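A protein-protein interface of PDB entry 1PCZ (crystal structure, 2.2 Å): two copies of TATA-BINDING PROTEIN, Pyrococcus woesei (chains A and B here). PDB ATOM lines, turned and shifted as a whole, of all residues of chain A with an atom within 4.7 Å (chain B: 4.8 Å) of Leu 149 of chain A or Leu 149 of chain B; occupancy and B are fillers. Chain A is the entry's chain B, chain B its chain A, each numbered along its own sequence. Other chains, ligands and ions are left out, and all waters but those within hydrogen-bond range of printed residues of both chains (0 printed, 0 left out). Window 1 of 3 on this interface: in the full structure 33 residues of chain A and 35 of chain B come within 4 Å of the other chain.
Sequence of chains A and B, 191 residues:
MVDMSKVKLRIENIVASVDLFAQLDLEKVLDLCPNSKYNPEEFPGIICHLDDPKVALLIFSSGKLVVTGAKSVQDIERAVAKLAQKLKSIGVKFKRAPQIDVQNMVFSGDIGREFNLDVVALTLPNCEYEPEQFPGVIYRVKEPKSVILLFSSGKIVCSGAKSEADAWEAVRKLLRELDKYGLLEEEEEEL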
ATOM      1  N   PHE A 134     -24.272  -8.994 -18.234  1.00  0.00           N
ATOM      2  CA  PHE A 134     -24.158  -9.923 -17.132  1.00  0.00           C
ATOM      3  C   PHE A 134     -25.366 -10.832 -17.119  1.00  0.00           C
ATOM      4  O   PHE A 134     -26.462 -10.438 -17.525  1.00  0.00           O
ATOM      5  CB  PHE A 134     -23.989  -9.199 -15.775  1.00  0.00           C
ATOM      6  CG  PHE A 134     -25.200  -8.434 -15.319  1.00  0.00           C
ATOM      7  CD1 PHE A 134     -26.351  -9.102 -14.876  1.00  0.00           C
ATOM      8  CD2 PHE A 134     -25.199  -7.041 -15.337  1.00  0.00           C
ATOM      9  CE1 PHE A 134     -27.484  -8.402 -14.464  1.00  0.00           C
ATOM     10  CE2 PHE A 134     -26.326  -6.325 -14.924  1.00  0.00           C
ATOM     11  CZ  PHE A 134     -27.479  -7.015 -14.487  1.00  0.00           C
ATOM     12  N   PRO A 135     -25.148 -12.112 -16.802  1.00  0.00           N
ATOM     13  CA  PRO A 135     -26.312 -12.978 -16.777  1.00  0.00           C
ATOM     14  C   PRO A 135     -27.091 -12.806 -15.471  1.00  0.00           C
ATOM     15  O   PRO A 135     -26.547 -12.355 -14.459  1.00  0.00           O
ATOM     16  CB  PRO A 135     -25.693 -14.372 -16.926  1.00  0.00           C
ATOM     17  CG  PRO A 135     -24.367 -14.224 -16.318  1.00  0.00           C
ATOM     18  CD  PRO A 135     -23.908 -12.909 -16.840  1.00  0.00           C
ATOM     19  N   GLY A 136     -28.380 -13.117 -15.523  1.00  0.00           N
ATOM     20  CA  GLY A 136     -29.217 -13.030 -14.354  1.00  0.00           C
ATOM     21  C   GLY A 136     -29.666 -11.642 -14.032  1.00  0.00           C
ATOM     22  O   GLY A 136     -29.246 -10.673 -14.628  1.00  0.00           O
ATOM     23  N   VAL A 137     -30.548 -11.554 -13.059  1.00  0.00           N
ATOM     24  CA  VAL A 137     -31.078 -10.287 -12.615  1.00  0.00           C
ATOM     25  C   VAL A 137     -30.432 -10.035 -11.258  1.00  0.00           C
ATOM     26  O   VAL A 137     -30.319 -10.934 -10.424  1.00  0.00           O
ATOM     27  CB  VAL A 137     -32.638 -10.365 -12.471  1.00  0.00           C
ATOM     28  CG1 VAL A 137     -33.169  -9.157 -11.731  1.00  0.00           C
ATOM     29  CG2 VAL A 137     -33.291 -10.462 -13.842  1.00  0.00           C
ATOM     30  N   ILE A 138     -29.989  -8.811 -11.062  1.00  0.00           N
ATOM     31  CA  ILE A 138     -29.364  -8.389  -9.825  1.00  0.00           C
ATOM     32  C   ILE A 138     -30.446  -7.777  -8.973  1.00  0.00           C
ATOM     33  O   ILE A 138     -31.161  -6.878  -9.404  1.00  0.00           O
ATOM     34  CB  ILE A 138     -28.297  -7.332 -10.089  1.00  0.00           C
ATOM     35  CG1 ILE A 138     -27.159  -7.941 -10.886  1.00  0.00           C
ATOM     36  CG2 ILE A 138     -27.771  -6.791  -8.814  1.00  0.00           C
ATOM     37  CD1 ILE A 138     -26.102  -6.936 -11.225  1.00  0.00           C
ATOM     38  N   VAL A 147     -26.819  -8.688  -2.240  1.00  0.00           N
ATOM     39  CA  VAL A 147     -27.137  -8.688  -3.646  1.00  0.00           C
ATOM     40  C   VAL A 147     -27.481 -10.103  -4.000  1.00  0.00           C
ATOM     41  O   VAL A 147     -26.769 -11.031  -3.611  1.00  0.00           O
ATOM     42  CB  VAL A 147     -25.930  -8.213  -4.494  1.00  0.00           C
ATOM     43  CG1 VAL A 147     -24.686  -9.029  -4.181  1.00  0.00           C
ATOM     44  CG2 VAL A 147     -26.260  -8.267  -5.960  1.00  0.00           C
ATOM     45  N   ILE A 148     -28.644 -10.281  -4.613  1.00  0.00           N
ATOM     46  CA  ILE A 148     -29.043 -11.586  -5.068  1.00  0.00           C
ATOM     47  C   ILE A 148     -29.078 -11.565  -6.572  1.00  0.00           C
ATOM     48  O   ILE A 148     -29.605 -10.658  -7.191  1.00  0.00           O
ATOM     49  CB  ILE A 148     -30.386 -12.027  -4.536  1.00  0.00           C
ATOM     50  CG1 ILE A 148     -30.308 -12.218  -3.032  1.00  0.00           C
ATOM     51  CG2 ILE A 148     -30.754 -13.358  -5.155  1.00  0.00           C
ATOM     52  CD1 ILE A 148     -31.599 -12.493  -2.447  1.00  0.00           C
ATOM     53  N   LEU A 149     -28.395 -12.516  -7.160  1.00  0.00           N
ATOM     54  CA  LEU A 149     -28.373 -12.617  -8.583  1.00  0.00           C
ATOM     55  C   LEU A 149     -29.346 -13.752  -8.863  1.00  0.00           C
ATOM     56  O   LEU A 149     -29.202 -14.836  -8.301  1.00  0.00           O
ATOM     57  CB  LEU A 149     -26.960 -12.941  -9.034  1.00  0.00           C
ATOM     58  CG  LEU A 149     -26.696 -13.120 -10.519  1.00  0.00           C
ATOM     59  CD1 LEU A 149     -27.241 -11.951 -11.370  1.00  0.00           C
ATOM     60  CD2 LEU A 149     -25.198 -13.282 -10.640  1.00  0.00           C
ATOM     61  N   LEU A 150     -30.393 -13.457  -9.635  1.00  0.00           N
ATOM     62  CA  LEU A 150     -31.418 -14.436  -9.966  1.00  0.00           C
ATOM     63  C   LEU A 150     -31.295 -14.877 -11.398  1.00  0.00           C
ATOM     64  O   LEU A 150     -31.111 -14.070 -12.297  1.00  0.00           O
ATOM     65  CB  LEU A 150     -32.826 -13.863  -9.706  1.00  0.00           C
ATOM     66  CG  LEU A 150     -34.057 -14.663 -10.189  1.00  0.00           C
ATOM     67  CD1 LEU A 150     -34.244 -15.942  -9.394  1.00  0.00           C
ATOM     68  CD2 LEU A 150     -35.295 -13.803 -10.102  1.00  0.00           C
ATOM     69  N   PHE A 151     -31.350 -16.183 -11.597  1.00  0.00           N
ATOM     70  CA  PHE A 151     -31.279 -16.757 -12.921  1.00  0.00           C
ATOM     71  C   PHE A 151     -32.638 -17.317 -13.285  1.00  0.00           C
ATOM     72  O   PHE A 151     -33.422 -17.656 -12.406  1.00  0.00           O
ATOM     73  CB  PHE A 151     -30.214 -17.840 -12.935  1.00  0.00           C
ATOM     74  CG  PHE A 151     -28.864 -17.297 -12.657  1.00  0.00           C
ATOM     75  CD1 PHE A 151     -28.256 -16.455 -13.580  1.00  0.00           C
ATOM     76  CD2 PHE A 151     -28.252 -17.515 -11.431  1.00  0.00           C
ATOM     77  CE1 PHE A 151     -27.084 -15.837 -13.288  1.00  0.00           C
ATOM     78  CE2 PHE A 151     -27.070 -16.902 -11.125  1.00  0.00           C
ATOM     79  CZ  PHE A 151     -26.483 -16.061 -12.048  1.00  0.00           C
ATOM     80  N   LYS A 155     -32.221 -20.453  -9.866  1.00  0.00           N
ATOM     81  CA  LYS A 155     -31.007 -20.527  -9.103  1.00  0.00           C
ATOM     82  C   LYS A 155     -30.639 -19.088  -8.783  1.00  0.00           C
ATOM     83  O   LYS A 155     -30.845 -18.174  -9.598  1.00  0.00           O
ATOM     84  CB  LYS A 155     -29.905 -21.188  -9.903  1.00  0.00           C
ATOM     85  CG  LYS A 155     -30.248 -22.597 -10.351  1.00  0.00           C
ATOM     86  CD  LYS A 155     -30.744 -23.443  -9.211  1.00  0.00           C
ATOM     87  CE  LYS A 155     -31.294 -24.774  -9.716  1.00  0.00           C
ATOM     88  NZ  LYS A 155     -32.595 -24.644 -10.461  1.00  0.00           N
ATOM     89  N   ILE A 156     -30.206 -18.873  -7.551  1.00  0.00           N
ATOM     90  CA  ILE A 156     -29.810 -17.560  -7.104  1.00  0.00           C
ATOM     91  C   ILE A 156     -28.444 -17.656  -6.462  1.00  0.00           C
ATOM     92  O   ILE A 156     -27.996 -18.726  -6.070  1.00  0.00           O
ATOM     93  CB  ILE A 156     -30.784 -16.995  -6.053  1.00  0.00           C
ATOM     94  CG1 ILE A 156     -30.937 -18.002  -4.911  1.00  0.00           C
ATOM     95  CG2 ILE A 156     -32.136 -16.641  -6.710  1.00  0.00           C
ATOM     96  CD1 ILE A 156     -31.668 -17.493  -3.714  1.00  0.00           C
ATOM     97  N   VAL A 157     -27.766 -16.530  -6.404  1.00  0.00           N
ATOM     98  CA  VAL A 157     -26.490 -16.469  -5.747  1.00  0.00           C
ATOM     99  C   VAL A 157     -26.574 -15.220  -4.908  1.00  0.00           C
ATOM    100  O   VAL A 157     -26.663 -14.116  -5.458  1.00  0.00           O
ATOM    101  CB  VAL A 157     -25.332 -16.339  -6.724  1.00  0.00           C
ATOM    102  CG1 VAL A 157     -24.012 -16.311  -5.963  1.00  0.00           C
ATOM    103  CG2 VAL A 157     -25.344 -17.480  -7.665  1.00  0.00           C
ATOM    104  N   PHE B 134     -21.491  -7.852  -6.888  1.00  0.00           N
ATOM    105  CA  PHE B 134     -22.021  -8.804  -7.826  1.00  0.00           C
ATOM    106  C   PHE B 134     -21.331 -10.109  -7.559  1.00  0.00           C
ATOM    107  O   PHE B 134     -20.111 -10.165  -7.556  1.00  0.00           O
ATOM    108  CB  PHE B 134     -21.693  -8.315  -9.247  1.00  0.00           C
ATOM    109  CG  PHE B 134     -22.319  -9.135 -10.337  1.00  0.00           C
ATOM    110  CD1 PHE B 134     -21.665 -10.243 -10.858  1.00  0.00           C
ATOM    111  CD2 PHE B 134     -23.566  -8.792 -10.856  1.00  0.00           C
ATOM    112  CE1 PHE B 134     -22.236 -10.986 -11.861  1.00  0.00           C
ATOM    113  CE2 PHE B 134     -24.143  -9.546 -11.874  1.00  0.00           C
ATOM    114  CZ  PHE B 134     -23.476 -10.639 -12.375  1.00  0.00           C
ATOM    115  N   PRO B 135     -22.098 -11.180  -7.330  1.00  0.00           N
ATOM    116  CA  PRO B 135     -21.423 -12.451  -7.076  1.00  0.00           C
ATOM    117  C   PRO B 135     -20.760 -13.018  -8.314  1.00  0.00           C
ATOM    118  O   PRO B 135     -21.195 -12.770  -9.438  1.00  0.00           O
ATOM    119  CB  PRO B 135     -22.559 -13.356  -6.584  1.00  0.00           C
ATOM    120  CG  PRO B 135     -23.764 -12.795  -7.235  1.00  0.00           C
ATOM    121  CD  PRO B 135     -23.553 -11.306  -7.111  1.00  0.00           C
ATOM    122  N   GLY B 136     -19.657 -13.724  -8.096  1.00  0.00           N
ATOM    123  CA  GLY B 136     -18.969 -14.377  -9.180  1.00  0.00           C
ATOM    124  C   GLY B 136     -17.945 -13.502  -9.830  1.00  0.00           C
ATOM    125  O   GLY B 136     -17.826 -12.324  -9.512  1.00  0.00           O
ATOM    126  N   VAL B 137     -17.125 -14.140 -10.654  1.00  0.00           N
ATOM    127  CA  VAL B 137     -16.082 -13.493 -11.423  1.00  0.00           C
ATOM    128  C   VAL B 137     -16.699 -13.374 -12.808  1.00  0.00           C
ATOM    129  O   VAL B 137     -17.227 -14.345 -13.357  1.00  0.00           O
ATOM    130  CB  VAL B 137     -14.788 -14.391 -11.533  1.00  0.00           C
ATOM    131  CG1 VAL B 137     -13.869 -13.859 -12.613  1.00  0.00           C
ATOM    132  CG2 VAL B 137     -14.052 -14.463 -10.204  1.00  0.00           C
ATOM    133  N   ILE B 138     -16.680 -12.166 -13.336  1.00  0.00           N
ATOM    134  CA  ILE B 138     -17.205 -11.872 -14.654  1.00  0.00           C
ATOM    135  C   ILE B 138     -16.076 -11.981 -15.647  1.00  0.00           C
ATOM    136  O   ILE B 138     -15.053 -11.315 -15.511  1.00  0.00           O
ATOM    137  CB  ILE B 138     -17.768 -10.463 -14.699  1.00  0.00           C
ATOM    138  CG1 ILE B 138     -19.112 -10.430 -13.992  1.00  0.00           C
ATOM    139  CG2 ILE B 138     -17.911 -10.002 -16.093  1.00  0.00           C
ATOM    140  CD1 ILE B 138     -19.730  -9.050 -13.965  1.00  0.00           C
ATOM    141  N   VAL B 147     -20.180 -13.127 -21.989  1.00  0.00           N
ATOM    142  CA  VAL B 147     -19.698 -12.936 -20.652  1.00  0.00           C
ATOM    143  C   VAL B 147     -20.006 -14.210 -19.899  1.00  0.00           C
ATOM    144  O   VAL B 147     -21.068 -14.827 -20.078  1.00  0.00           O
ATOM    145  CB  VAL B 147     -20.380 -11.738 -19.979  1.00  0.00           C
ATOM    146  CG1 VAL B 147     -21.921 -11.872 -20.053  1.00  0.00           C
ATOM    147  CG2 VAL B 147     -19.880 -11.612 -18.568  1.00  0.00           C
ATOM    148  N   ILE B 148     -19.028 -14.660 -19.139  1.00  0.00           N
ATOM    149  CA  ILE B 148     -19.198 -15.836 -18.339  1.00  0.00           C
ATOM    150  C   ILE B 148     -19.150 -15.348 -16.908  1.00  0.00           C
ATOM    151  O   ILE B 148     -18.412 -14.447 -16.564  1.00  0.00           O
ATOM    152  CB  ILE B 148     -18.085 -16.844 -18.591  1.00  0.00           C
ATOM    153  CG1 ILE B 148     -18.052 -17.219 -20.068  1.00  0.00           C
ATOM    154  CG2 ILE B 148     -18.315 -18.098 -17.768  1.00  0.00           C
ATOM    155  CD1 ILE B 148     -16.970 -18.202 -20.394  1.00  0.00           C
ATOM    156  N   LEU B 149     -20.032 -15.868 -16.099  1.00  0.00           N
ATOM    157  CA  LEU B 149     -20.068 -15.510 -14.711  1.00  0.00           C
ATOM    158  C   LEU B 149     -19.607 -16.805 -14.088  1.00  0.00           C
ATOM    159  O   LEU B 149     -20.198 -17.848 -14.338  1.00  0.00           O
ATOM    160  CB  LEU B 149     -21.505 -15.174 -14.326  1.00  0.00           C
ATOM    161  CG  LEU B 149     -21.819 -14.830 -12.884  1.00  0.00           C
ATOM    162  CD1 LEU B 149     -20.750 -13.910 -12.278  1.00  0.00           C
ATOM    163  CD2 LEU B 149     -23.195 -14.210 -12.884  1.00  0.00           C
ATOM    164  N   LEU B 150     -18.481 -16.751 -13.398  1.00  0.00           N
ATOM    165  CA  LEU B 150     -17.899 -17.932 -12.775  1.00  0.00           C
ATOM    166  C   LEU B 150     -18.128 -17.849 -11.292  1.00  0.00           C
ATOM    167  O   LEU B 150     -17.851 -16.826 -10.658  1.00  0.00           O
ATOM    168  CB  LEU B 150     -16.388 -17.952 -13.009  1.00  0.00           C
ATOM    169  CG  LEU B 150     -15.517 -19.208 -13.065  1.00  0.00           C
ATOM    170  CD1 LEU B 150     -14.107 -18.860 -12.592  1.00  0.00           C
ATOM    171  CD2 LEU B 150     -16.084 -20.331 -12.283  1.00  0.00           C
ATOM    172  N   PHE B 151     -18.616 -18.936 -10.726  1.00  0.00           N
ATOM    173  CA  PHE B 151     -18.841 -19.001  -9.304  1.00  0.00           C
ATOM    174  C   PHE B 151     -17.824 -19.936  -8.661  1.00  0.00           C
ATOM    175  O   PHE B 151     -17.242 -20.805  -9.314  1.00  0.00           O
ATOM    176  CB  PHE B 151     -20.264 -19.456  -9.061  1.00  0.00           C
ATOM    177  CG  PHE B 151     -21.270 -18.463  -9.546  1.00  0.00           C
ATOM    178  CD1 PHE B 151     -21.346 -17.212  -8.969  1.00  0.00           C
ATOM    179  CD2 PHE B 151     -22.117 -18.766 -10.607  1.00  0.00           C
ATOM    180  CE1 PHE B 151     -22.240 -16.287  -9.434  1.00  0.00           C
ATOM    181  CE2 PHE B 151     -23.016 -17.845 -11.078  1.00  0.00           C
ATOM    182  CZ  PHE B 151     -23.080 -16.605 -10.494  1.00  0.00           C
ATOM    183  N   LYS B 155     -19.865 -23.399 -11.017  1.00  0.00           N
ATOM    184  CA  LYS B 155     -21.003 -23.176 -11.881  1.00  0.00           C
ATOM    185  C   LYS B 155     -20.689 -21.904 -12.581  1.00  0.00           C
ATOM    186  O   LYS B 155     -20.089 -20.971 -12.018  1.00  0.00           O
ATOM    187  CB  LYS B 155     -22.299 -22.987 -11.108  1.00  0.00           C
ATOM    188  CG  LYS B 155     -22.665 -24.167 -10.223  1.00  0.00           C
ATOM    189  CD  LYS B 155     -22.689 -25.487 -10.964  1.00  0.00           C
ATOM    190  CE  LYS B 155     -22.873 -26.634  -9.971  1.00  0.00           C
ATOM    191  NZ  LYS B 155     -21.732 -26.708  -8.973  1.00  0.00           N
ATOM    192  N   ILE B 156     -21.040 -21.889 -13.844  1.00  0.00           N
ATOM    193  CA  ILE B 156     -20.845 -20.714 -14.666  1.00  0.00           C
ATOM    194  C   ILE B 156     -22.197 -20.365 -15.339  1.00  0.00           C
ATOM    195  O   ILE B 156     -23.129 -21.175 -15.382  1.00  0.00           O
ATOM    196  CB  ILE B 156     -19.765 -20.987 -15.749  1.00  0.00           C
ATOM    197  CG1 ILE B 156     -20.158 -22.217 -16.565  1.00  0.00           C
ATOM    198  CG2 ILE B 156     -18.413 -21.227 -15.095  1.00  0.00           C
ATOM    199  CD1 ILE B 156     -19.352 -22.417 -17.779  1.00  0.00           C
ATOM    200  N   VAL B 157     -22.331 -19.124 -15.753  1.00  0.00           N
ATOM    201  CA  VAL B 157     -23.505 -18.709 -16.487  1.00  0.00           C
ATOM    202  C   VAL B 157     -22.946 -17.880 -17.607  1.00  0.00           C
ATOM    203  O   VAL B 157     -22.215 -16.934 -17.369  1.00  0.00           O
ATOM    204  CB  VAL B 157     -24.483 -17.885 -15.679  1.00  0.00           C
ATOM    205  CG1 VAL B 157     -25.692 -17.566 -16.552  1.00  0.00           C
ATOM    206  CG2 VAL B 157     -24.915 -18.661 -14.452  1.00  0.00           C
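CZ of Phe 134 of chain B touches CB of Phe 134 of chain A, 3.7 Å away. CB of Leu 149 of chain B touches CG of Pro 135 of chain A (3.6 Å). CB of Pro 135 of chain A touches CG1 of Val 157 of chain B, at 3.2 Å. Phe 134 of chain B touches Ile 138 of chain A. CG1 of Val 147 of chain A touches CD of Pro 135 of chain B, at 3.9 Å. Phe 134 of chain B touches Leu 149 of chain A. Leu 149 of chain A touches Leu 149 of chain B (CD2 to CD2, 3.1 Å). Phe 151 of chain A touches Leu 149 of chain B. Phe 151 of chain B touches Phe 151 of chain A (CZ to CZ, 3.8 Å). CG2 of Val 157 of chain A touches CZ of Phe 151 of chain B, at 3.7 Å.
Phe 134 of chain B touches its own counterpart, Phe 134 of chain A. Leu 149 of chain A touches Phe 151 of chain B, and with the chains exchanged Phe 151 of chain A touches Leu 149 of chain B. Phe 151 of chain B touches its own counterpart, Phe 151 of chain A. Phe 151 of chain A touches Val 157 of chain B, and with the chains exchanged Val 157 of chain A touches Phe 151 of chain B. Positions printed for both chains: 134, 135, 136, 137, 138, 147, 148, 149, 150, 151, 155, 156 and 157.
Leu 149 of chain A touches just these residues of chain B: Phe 134, Pro 135, Leu 149 and Phe 151. Lys 155 of chain A touches none of the printed residues of chain B. Of the printed residues of chain A, Val 147 of chain B touches Pro 135. Leu 149 of chain B touches just these residues of chain A: Pro 135, Leu 149 and Phe 151. Of the printed residues of chain A, Phe 151 of chain B touches Leu 149, Phe 151 and Val 157. The nearest printed residue of chain B that does not touch Leu 149 of chain A is Gly 136 of chain B (6.1 Å). The nearest printed residue of chain A that does not touch Leu 149 of chain B is Phe 134 of chain A (5.8 Å). The nearest printed residue of chain A that does not touch Val 157 of chain B is Gly 136 of chain A (5.3 Å).
Hydrophobic or aromatic side chains of chain A that line the printed part of chain B: Phe 134, Pro 135, Ile 138, Val 147, Leu 149, Phe 151 and Val 157. Along chain A the printed residues that touch a printed residue of chain B span positions 134 to 157. Hydrophobic or aromatic side chains of chain B that line the printed part of chain A: Phe 134, Pro 135, Val 147, Leu 149, Phe 151 and Val 157. Among the printed residues, 15 pairs touch across the chains. Among the printed residues, no Asp or Glu carboxylate lies within 4 Å of a Lys or Arg side-chain nitrogen of the other chain.
The backbone carbonyl oxygen of Val 157 of chain B lies within hydrogen-bond range of the backbone NH of Leu 149 of chain B (2.7 Å). The backbone carbonyl oxygen of Val 157 of chain A lies within hydrogen-bond range of the backbone NH of Leu 149 of chain A, 2.9 Å away.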
